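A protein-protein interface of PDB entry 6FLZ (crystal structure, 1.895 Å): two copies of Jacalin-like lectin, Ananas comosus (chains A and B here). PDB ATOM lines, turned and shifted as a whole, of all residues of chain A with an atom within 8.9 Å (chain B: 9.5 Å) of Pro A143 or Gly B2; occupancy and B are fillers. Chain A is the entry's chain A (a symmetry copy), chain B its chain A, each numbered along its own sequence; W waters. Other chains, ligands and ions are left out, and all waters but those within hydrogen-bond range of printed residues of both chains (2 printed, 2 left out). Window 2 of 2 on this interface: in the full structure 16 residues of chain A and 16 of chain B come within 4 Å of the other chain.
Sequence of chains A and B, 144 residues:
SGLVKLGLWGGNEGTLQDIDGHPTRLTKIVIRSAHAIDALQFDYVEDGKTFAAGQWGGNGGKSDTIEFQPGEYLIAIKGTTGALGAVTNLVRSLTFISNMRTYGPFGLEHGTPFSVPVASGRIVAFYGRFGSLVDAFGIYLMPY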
ATOM      1  N   SER A   1     -13.880 -20.673   5.581  1.00  0.00           N
ATOM      2  CA  SER A   1     -14.196 -19.361   5.019  1.00  0.00           C
ATOM      3  C   SER A   1     -13.305 -19.036   3.830  1.00  0.00           C
ATOM      4  O   SER A   1     -12.192 -18.542   3.994  1.00  0.00           O
ATOM      5  CB  SER A   1     -14.050 -18.269   6.083  1.00  0.00           C
ATOM      6  OG  SER A   1     -14.177 -16.971   5.513  1.00  0.00           O
ATOM      7  N   GLY A   2     -13.801 -19.326   2.631  1.00  0.00           N
ATOM      8  CA  GLY A   2     -13.177 -18.841   1.416  1.00  0.00           C
ATOM      9  C   GLY A   2     -13.680 -17.462   1.028  1.00  0.00           C
ATOM     10  O   GLY A   2     -13.966 -17.202  -0.149  1.00  0.00           O
ATOM     11  N   LEU A   3     -13.790 -16.561   1.999  1.00  0.00           N
ATOM     12  CA  LEU A   3     -14.289 -15.220   1.748  1.00  0.00           C
ATOM     13  C   LEU A   3     -13.155 -14.206   1.837  1.00  0.00           C
ATOM     14  O   LEU A   3     -12.239 -14.343   2.656  1.00  0.00           O
ATOM     15  CB  LEU A   3     -15.395 -14.850   2.741  1.00  0.00           C
ATOM     16  CG  LEU A   3     -16.615 -15.772   2.775  1.00  0.00           C
ATOM     17  CD1 LEU A   3     -17.554 -15.360   3.894  1.00  0.00           C
ATOM     18  CD2 LEU A   3     -17.338 -15.762   1.441  1.00  0.00           C
ATOM     19  N   VAL A   4     -13.228 -13.190   0.989  1.00  0.00           N
ATOM     20  CA  VAL A   4     -12.372 -12.022   1.130  1.00  0.00           C
ATOM     21  C   VAL A   4     -13.038 -11.083   2.124  1.00  0.00           C
ATOM     22  O   VAL A   4     -14.237 -10.796   2.018  1.00  0.00           O
ATOM     23  CB  VAL A   4     -12.151 -11.340  -0.230  1.00  0.00           C
ATOM     24  CG1 VAL A   4     -11.437  -9.998  -0.057  1.00  0.00           C
ATOM     25  CG2 VAL A   4     -11.363 -12.254  -1.164  1.00  0.00           C
ATOM     26  N   PRO A  23     -21.433 -17.587   5.324  1.00  0.00           N
ATOM     27  CA  PRO A  23     -22.532 -17.058   4.508  1.00  0.00           C
ATOM     28  C   PRO A  23     -22.266 -17.201   3.023  1.00  0.00           C
ATOM     29  O   PRO A  23     -21.144 -17.007   2.553  1.00  0.00           O
ATOM     30  CB  PRO A  23     -22.591 -15.580   4.911  1.00  0.00           C
ATOM     31  CG  PRO A  23     -21.232 -15.281   5.414  1.00  0.00           C
ATOM     32  CD  PRO A  23     -20.744 -16.522   6.073  1.00  0.00           C
ATOM     33  N   THR A  24     -23.327 -17.514   2.281  1.00  0.00           N
ATOM     34  CA  THR A  24     -23.270 -17.570   0.831  1.00  0.00           C
ATOM     35  C   THR A  24     -24.284 -16.656   0.167  1.00  0.00           C
ATOM     36  O   THR A  24     -24.293 -16.559  -1.063  1.00  0.00           O
ATOM     37  CB  THR A  24     -23.498 -19.007   0.346  1.00  0.00           C
ATOM     38  OG1 THR A  24     -24.796 -19.440   0.763  1.00  0.00           O
ATOM     39  CG2 THR A  24     -22.442 -19.928   0.917  1.00  0.00           C
ATOM     40  N   VAL A 118     -17.894  -3.464  -6.912  1.00  0.00           N
ATOM     41  CA  VAL A 118     -17.596  -4.882  -7.102  1.00  0.00           C
ATOM     42  C   VAL A 118     -17.776  -5.189  -8.580  1.00  0.00           C
ATOM     43  O   VAL A 118     -18.901  -5.170  -9.094  1.00  0.00           O
ATOM     44  CB  VAL A 118     -18.485  -5.774  -6.224  1.00  0.00           C
ATOM     45  CG1 VAL A 118     -18.116  -7.254  -6.394  1.00  0.00           C
ATOM     46  CG2 VAL A 118     -18.369  -5.349  -4.765  1.00  0.00           C
ATOM     47  N   SER A 120     -16.519  -8.192  -9.935  1.00  0.00           N
ATOM     48  CA  SER A 120     -16.843  -9.615  -9.953  1.00  0.00           C
ATOM     49  C   SER A 120     -16.819 -10.110  -8.518  1.00  0.00           C
ATOM     50  O   SER A 120     -15.784 -10.034  -7.850  1.00  0.00           O
ATOM     51  CB  SER A 120     -15.865 -10.411 -10.827  1.00  0.00           C
ATOM     52  OG  SER A 120     -16.268 -11.763 -10.934  1.00  0.00           O
ATOM     53  N   GLY A 121     -17.956 -10.588  -8.046  1.00  0.00           N
ATOM     54  CA  GLY A 121     -18.059 -11.117  -6.701  1.00  0.00           C
ATOM     55  C   GLY A 121     -19.438 -10.851  -6.137  1.00  0.00           C
ATOM     56  O   GLY A 121     -20.284 -10.222  -6.767  1.00  0.00           O
ATOM     57  N   ARG A 122     -19.639 -11.340  -4.916  1.00  0.00           N
ATOM     58  CA  ARG A 122     -20.896 -11.165  -4.199  1.00  0.00           C
ATOM     59  C   ARG A 122     -20.604 -10.758  -2.764  1.00  0.00           C
ATOM     60  O   ARG A 122     -19.794 -11.398  -2.083  1.00  0.00           O
ATOM     61  CB  ARG A 122     -21.746 -12.449  -4.216  1.00  0.00           C
ATOM     62  CG  ARG A 122     -22.355 -12.792  -5.573  1.00  0.00           C
ATOM     63  CD  ARG A 122     -23.360 -11.744  -6.010  1.00  0.00           C
ATOM     64  NE  ARG A 122     -24.022 -12.067  -7.272  1.00  0.00           N
ATOM     65  CZ  ARG A 122     -23.561 -11.739  -8.475  1.00  0.00           C
ATOM     66  NH1 ARG A 122     -22.412 -11.087  -8.603  1.00  0.00           N
ATOM     67  NH2 ARG A 122     -24.249 -12.069  -9.561  1.00  0.00           N
ATOM     68  N   ILE A 123     -21.273  -9.706  -2.308  1.00  0.00           N
ATOM     69  CA  ILE A 123     -21.213  -9.306  -0.905  1.00  0.00           C
ATOM     70  C   ILE A 123     -22.213 -10.163  -0.138  1.00  0.00           C
ATOM     71  O   ILE A 123     -23.403 -10.185  -0.473  1.00  0.00           O
ATOM     72  CB  ILE A 123     -21.520  -7.812  -0.746  1.00  0.00           C
ATOM     73  CG1 ILE A 123     -20.415  -6.983  -1.413  1.00  0.00           C
ATOM     74  CG2 ILE A 123     -21.699  -7.454   0.748  1.00  0.00           C
ATOM     75  CD1 ILE A 123     -20.750  -5.512  -1.559  1.00  0.00           C
ATOM     76  N   VAL A 124     -21.732 -10.878   0.880  1.00  0.00           N
ATOM     77  CA  VAL A 124     -22.555 -11.854   1.588  1.00  0.00           C
ATOM     78  C   VAL A 124     -22.720 -11.560   3.072  1.00  0.00           C
ATOM     79  O   VAL A 124     -23.599 -12.169   3.699  1.00  0.00           O
ATOM     80  CB  VAL A 124     -22.018 -13.289   1.398  1.00  0.00           C
ATOM     81  CG1 VAL A 124     -22.103 -13.705  -0.073  1.00  0.00           C
ATOM     82  CG2 VAL A 124     -20.595 -13.428   1.931  1.00  0.00           C
ATOM     83  N   TYR A 140     -17.720  -8.790   3.829  1.00  0.00           N
ATOM     84  CA  TYR A 140     -17.308 -10.106   3.347  1.00  0.00           C
ATOM     85  C   TYR A 140     -17.754 -10.308   1.905  1.00  0.00           C
ATOM     86  O   TYR A 140     -18.934 -10.117   1.595  1.00  0.00           O
ATOM     87  CB  TYR A 140     -17.925 -11.224   4.187  1.00  0.00           C
ATOM     88  CG  TYR A 140     -17.333 -11.450   5.533  1.00  0.00           C
ATOM     89  CD1 TYR A 140     -16.249 -12.293   5.690  1.00  0.00           C
ATOM     90  CD2 TYR A 140     -17.891 -10.869   6.667  1.00  0.00           C
ATOM     91  CE1 TYR A 140     -15.714 -12.547   6.947  1.00  0.00           C
ATOM     92  CE2 TYR A 140     -17.365 -11.112   7.927  1.00  0.00           C
ATOM     93  CZ  TYR A 140     -16.273 -11.956   8.058  1.00  0.00           C
ATOM     94  OH  TYR A 140     -15.738 -12.203   9.303  1.00  0.00           O
ATOM     95  N   LEU A 141     -16.829 -10.745   1.043  1.00  0.00           N
ATOM     96  CA  LEU A 141     -17.123 -11.028  -0.355  1.00  0.00           C
ATOM     97  C   LEU A 141     -16.736 -12.449  -0.737  1.00  0.00           C
ATOM     98  O   LEU A 141     -15.692 -12.961  -0.319  1.00  0.00           O
ATOM     99  CB  LEU A 141     -16.388 -10.067  -1.287  1.00  0.00           C
ATOM    100  CG  LEU A 141     -16.711  -8.596  -1.068  1.00  0.00           C
ATOM    101  CD1 LEU A 141     -15.648  -7.953  -0.189  1.00  0.00           C
ATOM    102  CD2 LEU A 141     -16.828  -7.888  -2.397  1.00  0.00           C
ATOM    103  N   MET A 142     -17.551 -13.038  -1.577  1.00  0.00           N
ATOM    104  CA  MET A 142     -17.404 -14.346  -2.184  1.00  0.00           C
ATOM    105  C   MET A 142     -17.071 -14.188  -3.663  1.00  0.00           C
ATOM    106  O   MET A 142     -17.654 -13.324  -4.332  1.00  0.00           O
ATOM    107  CB  MET A 142     -18.728 -15.102  -2.012  1.00  0.00           C
ATOM    108  CG  MET A 142     -18.815 -16.507  -2.467  1.00  0.00           C
ATOM    109  SD  MET A 142     -20.481 -17.111  -2.065  1.00  0.00           S
ATOM    110  CE  MET A 142     -21.533 -16.123  -3.121  1.00  0.00           C
ATOM    111  N   PRO A 143     -16.135 -14.967  -4.208  1.00  0.00           N
ATOM    112  CA  PRO A 143     -15.970 -14.973  -5.665  1.00  0.00           C
ATOM    113  C   PRO A 143     -17.275 -15.375  -6.331  1.00  0.00           C
ATOM    114  O   PRO A 143     -18.078 -16.119  -5.765  1.00  0.00           O
ATOM    115  CB  PRO A 143     -14.872 -16.017  -5.900  1.00  0.00           C
ATOM    116  CG  PRO A 143     -14.141 -16.100  -4.617  1.00  0.00           C
ATOM    117  CD  PRO A 143     -15.171 -15.869  -3.551  1.00  0.00           C
ATOM    118  N   TYR A 144     -17.505 -14.845  -7.529  1.00  0.00           N
ATOM    119  CA  TYR A 144     -18.727 -15.160  -8.269  1.00  0.00           C
ATOM    120  C   TYR A 144     -18.416 -16.050  -9.458  1.00  0.00           C
ATOM    121  O   TYR A 144     -17.524 -15.736 -10.241  1.00  0.00           O
ATOM    122  CB  TYR A 144     -19.425 -13.891  -8.742  1.00  0.00           C
ATOM    123  CG  TYR A 144     -20.678 -14.140  -9.556  1.00  0.00           C
ATOM    124  CD1 TYR A 144     -21.789 -14.753  -8.992  1.00  0.00           C
ATOM    125  CD2 TYR A 144     -20.757 -13.741 -10.887  1.00  0.00           C
ATOM    126  CE1 TYR A 144     -22.942 -14.973  -9.732  1.00  0.00           C
ATOM    127  CE2 TYR A 144     -21.903 -13.954 -11.635  1.00  0.00           C
ATOM    128  CZ  TYR A 144     -22.990 -14.569 -11.055  1.00  0.00           C
ATOM    129  OH  TYR A 144     -24.127 -14.781 -11.800  1.00  0.00           O
ATOM    130  OXT TYR A 144     -19.053 -17.082  -9.658  1.00  0.00           O
ATOM    131  N   SER B   1     -11.142 -18.384 -12.578  1.00  0.00           N
ATOM    132  CA  SER B   1     -10.855 -17.242 -11.710  1.00  0.00           C
ATOM    133  C   SER B   1     -11.749 -17.239 -10.481  1.00  0.00           C
ATOM    134  O   SER B   1     -12.874 -16.745 -10.522  1.00  0.00           O
ATOM    135  CB  SER B   1     -11.029 -15.927 -12.476  1.00  0.00           C
ATOM    136  OG  SER B   1     -10.930 -14.806 -11.605  1.00  0.00           O
ATOM    137  N   GLY B   2     -11.244 -17.802  -9.388  1.00  0.00           N
ATOM    138  CA  GLY B   2     -11.875 -17.644  -8.092  1.00  0.00           C
ATOM    139  C   GLY B   2     -11.402 -16.391  -7.378  1.00  0.00           C
ATOM    140  O   GLY B   2     -11.120 -16.420  -6.172  1.00  0.00           O
ATOM    141  N   LEU B   3     -11.316 -15.277  -8.099  1.00  0.00           N
ATOM    142  CA  LEU B   3     -10.847 -14.027  -7.525  1.00  0.00           C
ATOM    143  C   LEU B   3     -12.004 -13.048  -7.366  1.00  0.00           C
ATOM    144  O   LEU B   3     -12.919 -13.002  -8.196  1.00  0.00           O
ATOM    145  CB  LEU B   3      -9.753 -13.400  -8.394  1.00  0.00           C
ATOM    146  CG  LEU B   3      -8.512 -14.258  -8.650  1.00  0.00           C
ATOM    147  CD1 LEU B   3      -7.586 -13.563  -9.630  1.00  0.00           C
ATOM    148  CD2 LEU B   3      -7.786 -14.558  -7.351  1.00  0.00           C
ATOM    149  N   VAL B   4     -11.952 -12.270  -6.295  1.00  0.00           N
ATOM    150  CA  VAL B   4     -12.835 -11.122  -6.148  1.00  0.00           C
ATOM    151  C   VAL B   4     -12.193  -9.953  -6.881  1.00  0.00           C
ATOM    152  O   VAL B   4     -11.001  -9.674  -6.704  1.00  0.00           O
ATOM    153  CB  VAL B   4     -13.068 -10.800  -4.664  1.00  0.00           C
ATOM    154  CG1 VAL B   4     -13.812  -9.472  -4.505  1.00  0.00           C
ATOM    155  CG2 VAL B   4     -13.831 -11.932  -3.984  1.00  0.00           C
ATOM    156  N   LYS B   5     -12.974  -9.284  -7.720  1.00  0.00           N
ATOM    157  CA  LYS B   5     -12.488  -8.195  -8.564  1.00  0.00           C
ATOM    158  C   LYS B   5     -13.192  -6.912  -8.138  1.00  0.00           C
ATOM    159  O   LYS B   5     -14.413  -6.791  -8.292  1.00  0.00           O
ATOM    160  CB  LYS B   5     -12.755  -8.508 -10.033  1.00  0.00           C
ATOM    161  CG  LYS B   5     -12.106  -7.568 -11.046  1.00  0.00           C
ATOM    162  CD  LYS B   5     -12.487  -8.036 -12.450  1.00  0.00           C
ATOM    163  CE  LYS B   5     -11.828  -7.235 -13.534  1.00  0.00           C
ATOM    164  NZ  LYS B   5     -12.128  -7.821 -14.877  1.00  0.00           N
ATOM    165  N   GLY B  21      -5.093 -14.262 -17.197  1.00  0.00           N
ATOM    166  CA  GLY B  21      -4.414 -15.298 -16.444  1.00  0.00           C
ATOM    167  C   GLY B  21      -5.086 -15.551 -15.112  1.00  0.00           C
ATOM    168  O   GLY B  21      -6.178 -15.055 -14.833  1.00  0.00           O
ATOM    169  N   HIS B  22      -4.402 -16.346 -14.292  1.00  0.00           N
ATOM    170  CA  HIS B  22      -4.910 -16.799 -13.000  1.00  0.00           C
ATOM    171  C   HIS B  22      -3.840 -16.539 -11.943  1.00  0.00           C
ATOM    172  O   HIS B  22      -3.165 -17.460 -11.465  1.00  0.00           O
ATOM    173  CB  HIS B  22      -5.292 -18.277 -13.081  1.00  0.00           C
ATOM    174  CG  HIS B  22      -6.209 -18.588 -14.225  1.00  0.00           C
ATOM    175  ND1 HIS B  22      -7.565 -18.770 -14.066  1.00  0.00           N
ATOM    176  CD2 HIS B  22      -5.967 -18.711 -15.553  1.00  0.00           C
ATOM    177  CE1 HIS B  22      -8.116 -19.014 -15.242  1.00  0.00           C
ATOM    178  NE2 HIS B  22      -7.169 -18.981 -16.161  1.00  0.00           N
ATOM    179  N   PRO B  23      -3.662 -15.283 -11.551  1.00  0.00           N
ATOM    180  CA  PRO B  23      -2.572 -14.945 -10.628  1.00  0.00           C
ATOM    181  C   PRO B  23      -2.830 -15.453  -9.223  1.00  0.00           C
ATOM    182  O   PRO B  23      -3.955 -15.406  -8.723  1.00  0.00           O
ATOM    183  CB  PRO B  23      -2.548 -13.412 -10.657  1.00  0.00           C
ATOM    184  CG  PRO B  23      -3.915 -13.031 -11.075  1.00  0.00           C
ATOM    185  CD  PRO B  23      -4.376 -14.083 -12.019  1.00  0.00           C
ATOM    186  N   THR B  24      -1.760 -15.914  -8.578  1.00  0.00           N
ATOM    187  CA  THR B  24      -1.812 -16.324  -7.186  1.00  0.00           C
ATOM    188  C   THR B  24      -0.817 -15.578  -6.316  1.00  0.00           C
ATOM    189  O   THR B  24      -0.807 -15.785  -5.099  1.00  0.00           O
ATOM    190  CB  THR B  24      -1.550 -17.831  -7.067  1.00  0.00           C
ATOM    191  OG1 THR B  24      -0.244 -18.119  -7.573  1.00  0.00           O
ATOM    192  CG2 THR B  24      -2.586 -18.608  -7.849  1.00  0.00           C
ATOM    193  N   ARG B 122      -5.568 -11.776  -0.099  1.00  0.00           N
ATOM    194  CA  ARG B 122      -4.318 -11.402  -0.748  1.00  0.00           C
ATOM    195  C   ARG B 122      -4.623 -10.663  -2.040  1.00  0.00           C
ATOM    196  O   ARG B 122      -5.420 -11.135  -2.860  1.00  0.00           O
ATOM    197  CB  ARG B 122      -3.438 -12.632  -1.043  1.00  0.00           C
ATOM    198  CG  ARG B 122      -2.818 -13.281   0.190  1.00  0.00           C
ATOM    199  CD  ARG B 122      -1.836 -12.350   0.874  1.00  0.00           C
ATOM    200  NE  ARG B 122      -1.163 -12.958   2.020  1.00  0.00           N
ATOM    201  CZ  ARG B 122      -1.628 -12.945   3.266  1.00  0.00           C
ATOM    202  NH1 ARG B 122      -2.791 -12.370   3.546  1.00  0.00           N
ATOM    203  NH2 ARG B 122      -0.930 -13.514   4.240  1.00  0.00           N
ATOM    204  N   VAL B 124      -3.503  -9.861  -5.599  1.00  0.00           N
ATOM    205  CA  VAL B 124      -2.659 -10.615  -6.522  1.00  0.00           C
ATOM    206  C   VAL B 124      -2.506  -9.963  -7.889  1.00  0.00           C
ATOM    207  O   VAL B 124      -1.614 -10.379  -8.644  1.00  0.00           O
ATOM    208  CB  VAL B 124      -3.164 -12.065  -6.691  1.00  0.00           C
ATOM    209  CG1 VAL B 124      -3.065 -12.826  -5.367  1.00  0.00           C
ATOM    210  CG2 VAL B 124      -4.584 -12.101  -7.245  1.00  0.00           C
ATOM    211  N   TYR B 140      -7.570  -7.207  -7.959  1.00  0.00           N
ATOM    212  CA  TYR B 140      -7.951  -8.610  -7.815  1.00  0.00           C
ATOM    213  C   TYR B 140      -7.496  -9.148  -6.465  1.00  0.00           C
ATOM    214  O   TYR B 140      -6.319  -9.012  -6.114  1.00  0.00           O
ATOM    215  CB  TYR B 140      -7.310  -9.474  -8.901  1.00  0.00           C
ATOM    216  CG  TYR B 140      -7.901  -9.377 -10.263  1.00  0.00           C
ATOM    217  CD1 TYR B 140      -8.966 -10.180 -10.625  1.00  0.00           C
ATOM    218  CD2 TYR B 140      -7.359  -8.524 -11.219  1.00  0.00           C
ATOM    219  CE1 TYR B 140      -9.498 -10.131 -11.908  1.00  0.00           C
ATOM    220  CE2 TYR B 140      -7.883  -8.462 -12.502  1.00  0.00           C
ATOM    221  CZ  TYR B 140      -8.956  -9.273 -12.838  1.00  0.00           C
ATOM    222  OH  TYR B 140      -9.489  -9.220 -14.107  1.00  0.00           O
ATOM    223  N   LEU B 141      -8.408  -9.805  -5.739  1.00  0.00           N
ATOM    224  CA  LEU B 141      -8.103 -10.415  -4.452  1.00  0.00           C
ATOM    225  C   LEU B 141      -8.457 -11.894  -4.431  1.00  0.00           C
ATOM    226  O   LEU B 141      -9.490 -12.312  -4.964  1.00  0.00           O
ATOM    227  CB  LEU B 141      -8.858  -9.727  -3.315  1.00  0.00           C
ATOM    228  CG  LEU B 141      -8.569  -8.241  -3.166  1.00  0.00           C
ATOM    229  CD1 LEU B 141      -9.649  -7.427  -3.865  1.00  0.00           C
ATOM    230  CD2 LEU B 141      -8.464  -7.877  -1.704  1.00  0.00           C
ATOM    231  N   MET B 142      -7.627 -12.652  -3.758  1.00  0.00           N
ATOM    232  CA  MET B 142      -7.742 -14.071  -3.490  1.00  0.00           C
ATOM    233  C   MET B 142      -8.074 -14.288  -2.018  1.00  0.00           C
ATOM    234  O   MET B 142      -7.509 -13.601  -1.157  1.00  0.00           O
ATOM    235  CB  MET B 142      -6.401 -14.732  -3.838  1.00  0.00           C
ATOM    236  CG  MET B 142      -6.281 -16.203  -3.740  1.00  0.00           C
ATOM    237  SD  MET B 142      -4.603 -16.652  -4.273  1.00  0.00           S
ATOM    238  CE  MET B 142      -3.570 -15.929  -3.005  1.00  0.00           C
ATOM    239  N   PRO B 143      -8.991 -15.198  -1.683  1.00  0.00           N
ATOM    240  CA  PRO B 143      -9.151 -15.565  -0.272  1.00  0.00           C
ATOM    241  C   PRO B 143      -7.835 -16.088   0.279  1.00  0.00           C
ATOM    242  O   PRO B 143      -7.018 -16.652  -0.450  1.00  0.00           O
ATOM    243  CB  PRO B 143     -10.224 -16.659  -0.303  1.00  0.00           C
ATOM    244  CG  PRO B 143     -10.957 -16.442  -1.569  1.00  0.00           C
ATOM    245  CD  PRO B 143      -9.935 -15.933  -2.544  1.00  0.00           C
ATOM    246  N   TYR B 144      -7.614 -15.862   1.571  1.00  0.00           N
ATOM    247  CA  TYR B 144      -6.383 -16.321   2.214  1.00  0.00           C
ATOM    248  C   TYR B 144      -6.670 -17.481   3.148  1.00  0.00           C
ATOM    249  O   TYR B 144      -7.567 -17.389   3.982  1.00  0.00           O
ATOM    250  CB  TYR B 144      -5.713 -15.190   2.985  1.00  0.00           C
ATOM    251  CG  TYR B 144      -4.453 -15.602   3.718  1.00  0.00           C
ATOM    252  CD1 TYR B 144      -3.329 -16.033   3.023  1.00  0.00           C
ATOM    253  CD2 TYR B 144      -4.378 -15.539   5.106  1.00  0.00           C
ATOM    254  CE1 TYR B 144      -2.170 -16.401   3.690  1.00  0.00           C
ATOM    255  CE2 TYR B 144      -3.226 -15.902   5.782  1.00  0.00           C
ATOM    256  CZ  TYR B 144      -2.127 -16.332   5.072  1.00  0.00           C
ATOM    257  OH  TYR B 144      -0.983 -16.694   5.746  1.00  0.00           O
ATOM    258  OXT TYR B 144      -6.009 -18.515   3.091  1.00  0.00           O
HETATM  259  O   HOH W   1     -15.572 -13.338  -8.822  1.00  0.00           O
HETATM  260  O   HOH W   2      -9.578 -14.761   3.188  1.00  0.00           O
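Among the printed residues, pairs that only touch across the chains: Pro A143 with Gly B2 (3.4 Å), Gly A2 with Pro B143 (3.4 Å), Ser A120 with Val B4 (3.6 Å), Val A118 with Lys B5 (3.7 Å), Val A4 with Val B4 (3.8 Å), Val A4 with Pro B143 (3.8 Å), Pro A143 with Val B4 (3.8 Å), Val A4 with Met B142 (3.96 Å) and Met A142 with Val B4 (3.96 Å).
Gly A2 touches Pro B143, and with the chains exchanged Pro A143 touches Gly B2. Val A4 touches its own counterpart, Val B4. Val A4 touches Met B142, and with the chains exchanged Met A142 touches Val B4. Val A4 touches Pro B143, and with the chains exchanged Pro A143 touches Val B4.
N of Lys B5 sits at hydrogen-bond distance from O of Ser A120 (2.9 Å).
Water W1 lies within hydrogen-bond range of the side-chain hydroxyl (OG) of Ser A120 (2.7 Å), the backbone carbonyl oxygen (O) of Leu B3 (2.7 Å) and the backbone NH (N) of Tyr A144 (2.8 Å). Water W2 lies within hydrogen-bond range of the backbone carbonyl oxygen of Leu A3 (2.7 Å) and the backbone NH of Tyr B144 (2.8 Å).
Of the 16 printed residues of chain B, 5 touch a printed residue of chain A. Hydrophobic or aromatic side chains of chain B that line the printed part of chain A: Val B4 and Pro B143.
Of the printed residues of chain B, Val A4 touches Val B4 (3.8 Å), Met B142 (3.96 Å) and Pro B143 (3.8 Å). Pro A23 touches none of the printed residues of chain B. Gly A121 touches none of the printed residues of chain B. Of chain B, only Val B4 comes within 4 Å of Met A142. Pro A143 touches just these residues of chain B: Gly B2 (3.4 Å) and Val B4 (3.8 Å). No residue of chain A comes within 4 Å of Ser B1. Gly B2 touches just one residue of chain A: Pro A143 (3.4 Å). Of the printed residues of chain A, Val B4 touches Val A4, Ser A120, Met A142 and Pro A143. Printed residues of chain A within 4 Å of Met B142: Val A4 (3.96 Å). Printed residues of chain A within 4 Å of Pro B143: Gly A2 (3.4 Å) and Val A4 (3.8 Å). The nearest residue of chain B that does not touch Pro A143 is Leu B3 (4.2 Å). The nearest printed residue of chain A that does not touch Pro B143 is Leu A3 (4.2 Å).
The backbone carbonyl oxygen of Arg B122 is in hydrogen-bond range of the backbone NH of Met B142, 2.8 Å away. OH of Tyr B140 lies within hydrogen-bond range of NZ of Lys B5, 3.1 Å away. The backbone carbonyl oxygen (O) of Val A4 is in hydrogen-bond range of the backbone NH (N) of Leu A141 (2.8 Å). The backbone carbonyl oxygen (O) of Arg A122 is in hydrogen-bond range of the backbone NH (N) of Met A142, 2.8 Å away. O of Val B4 lies within hydrogen-bond range of N of Leu B141, 2.8 Å away.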
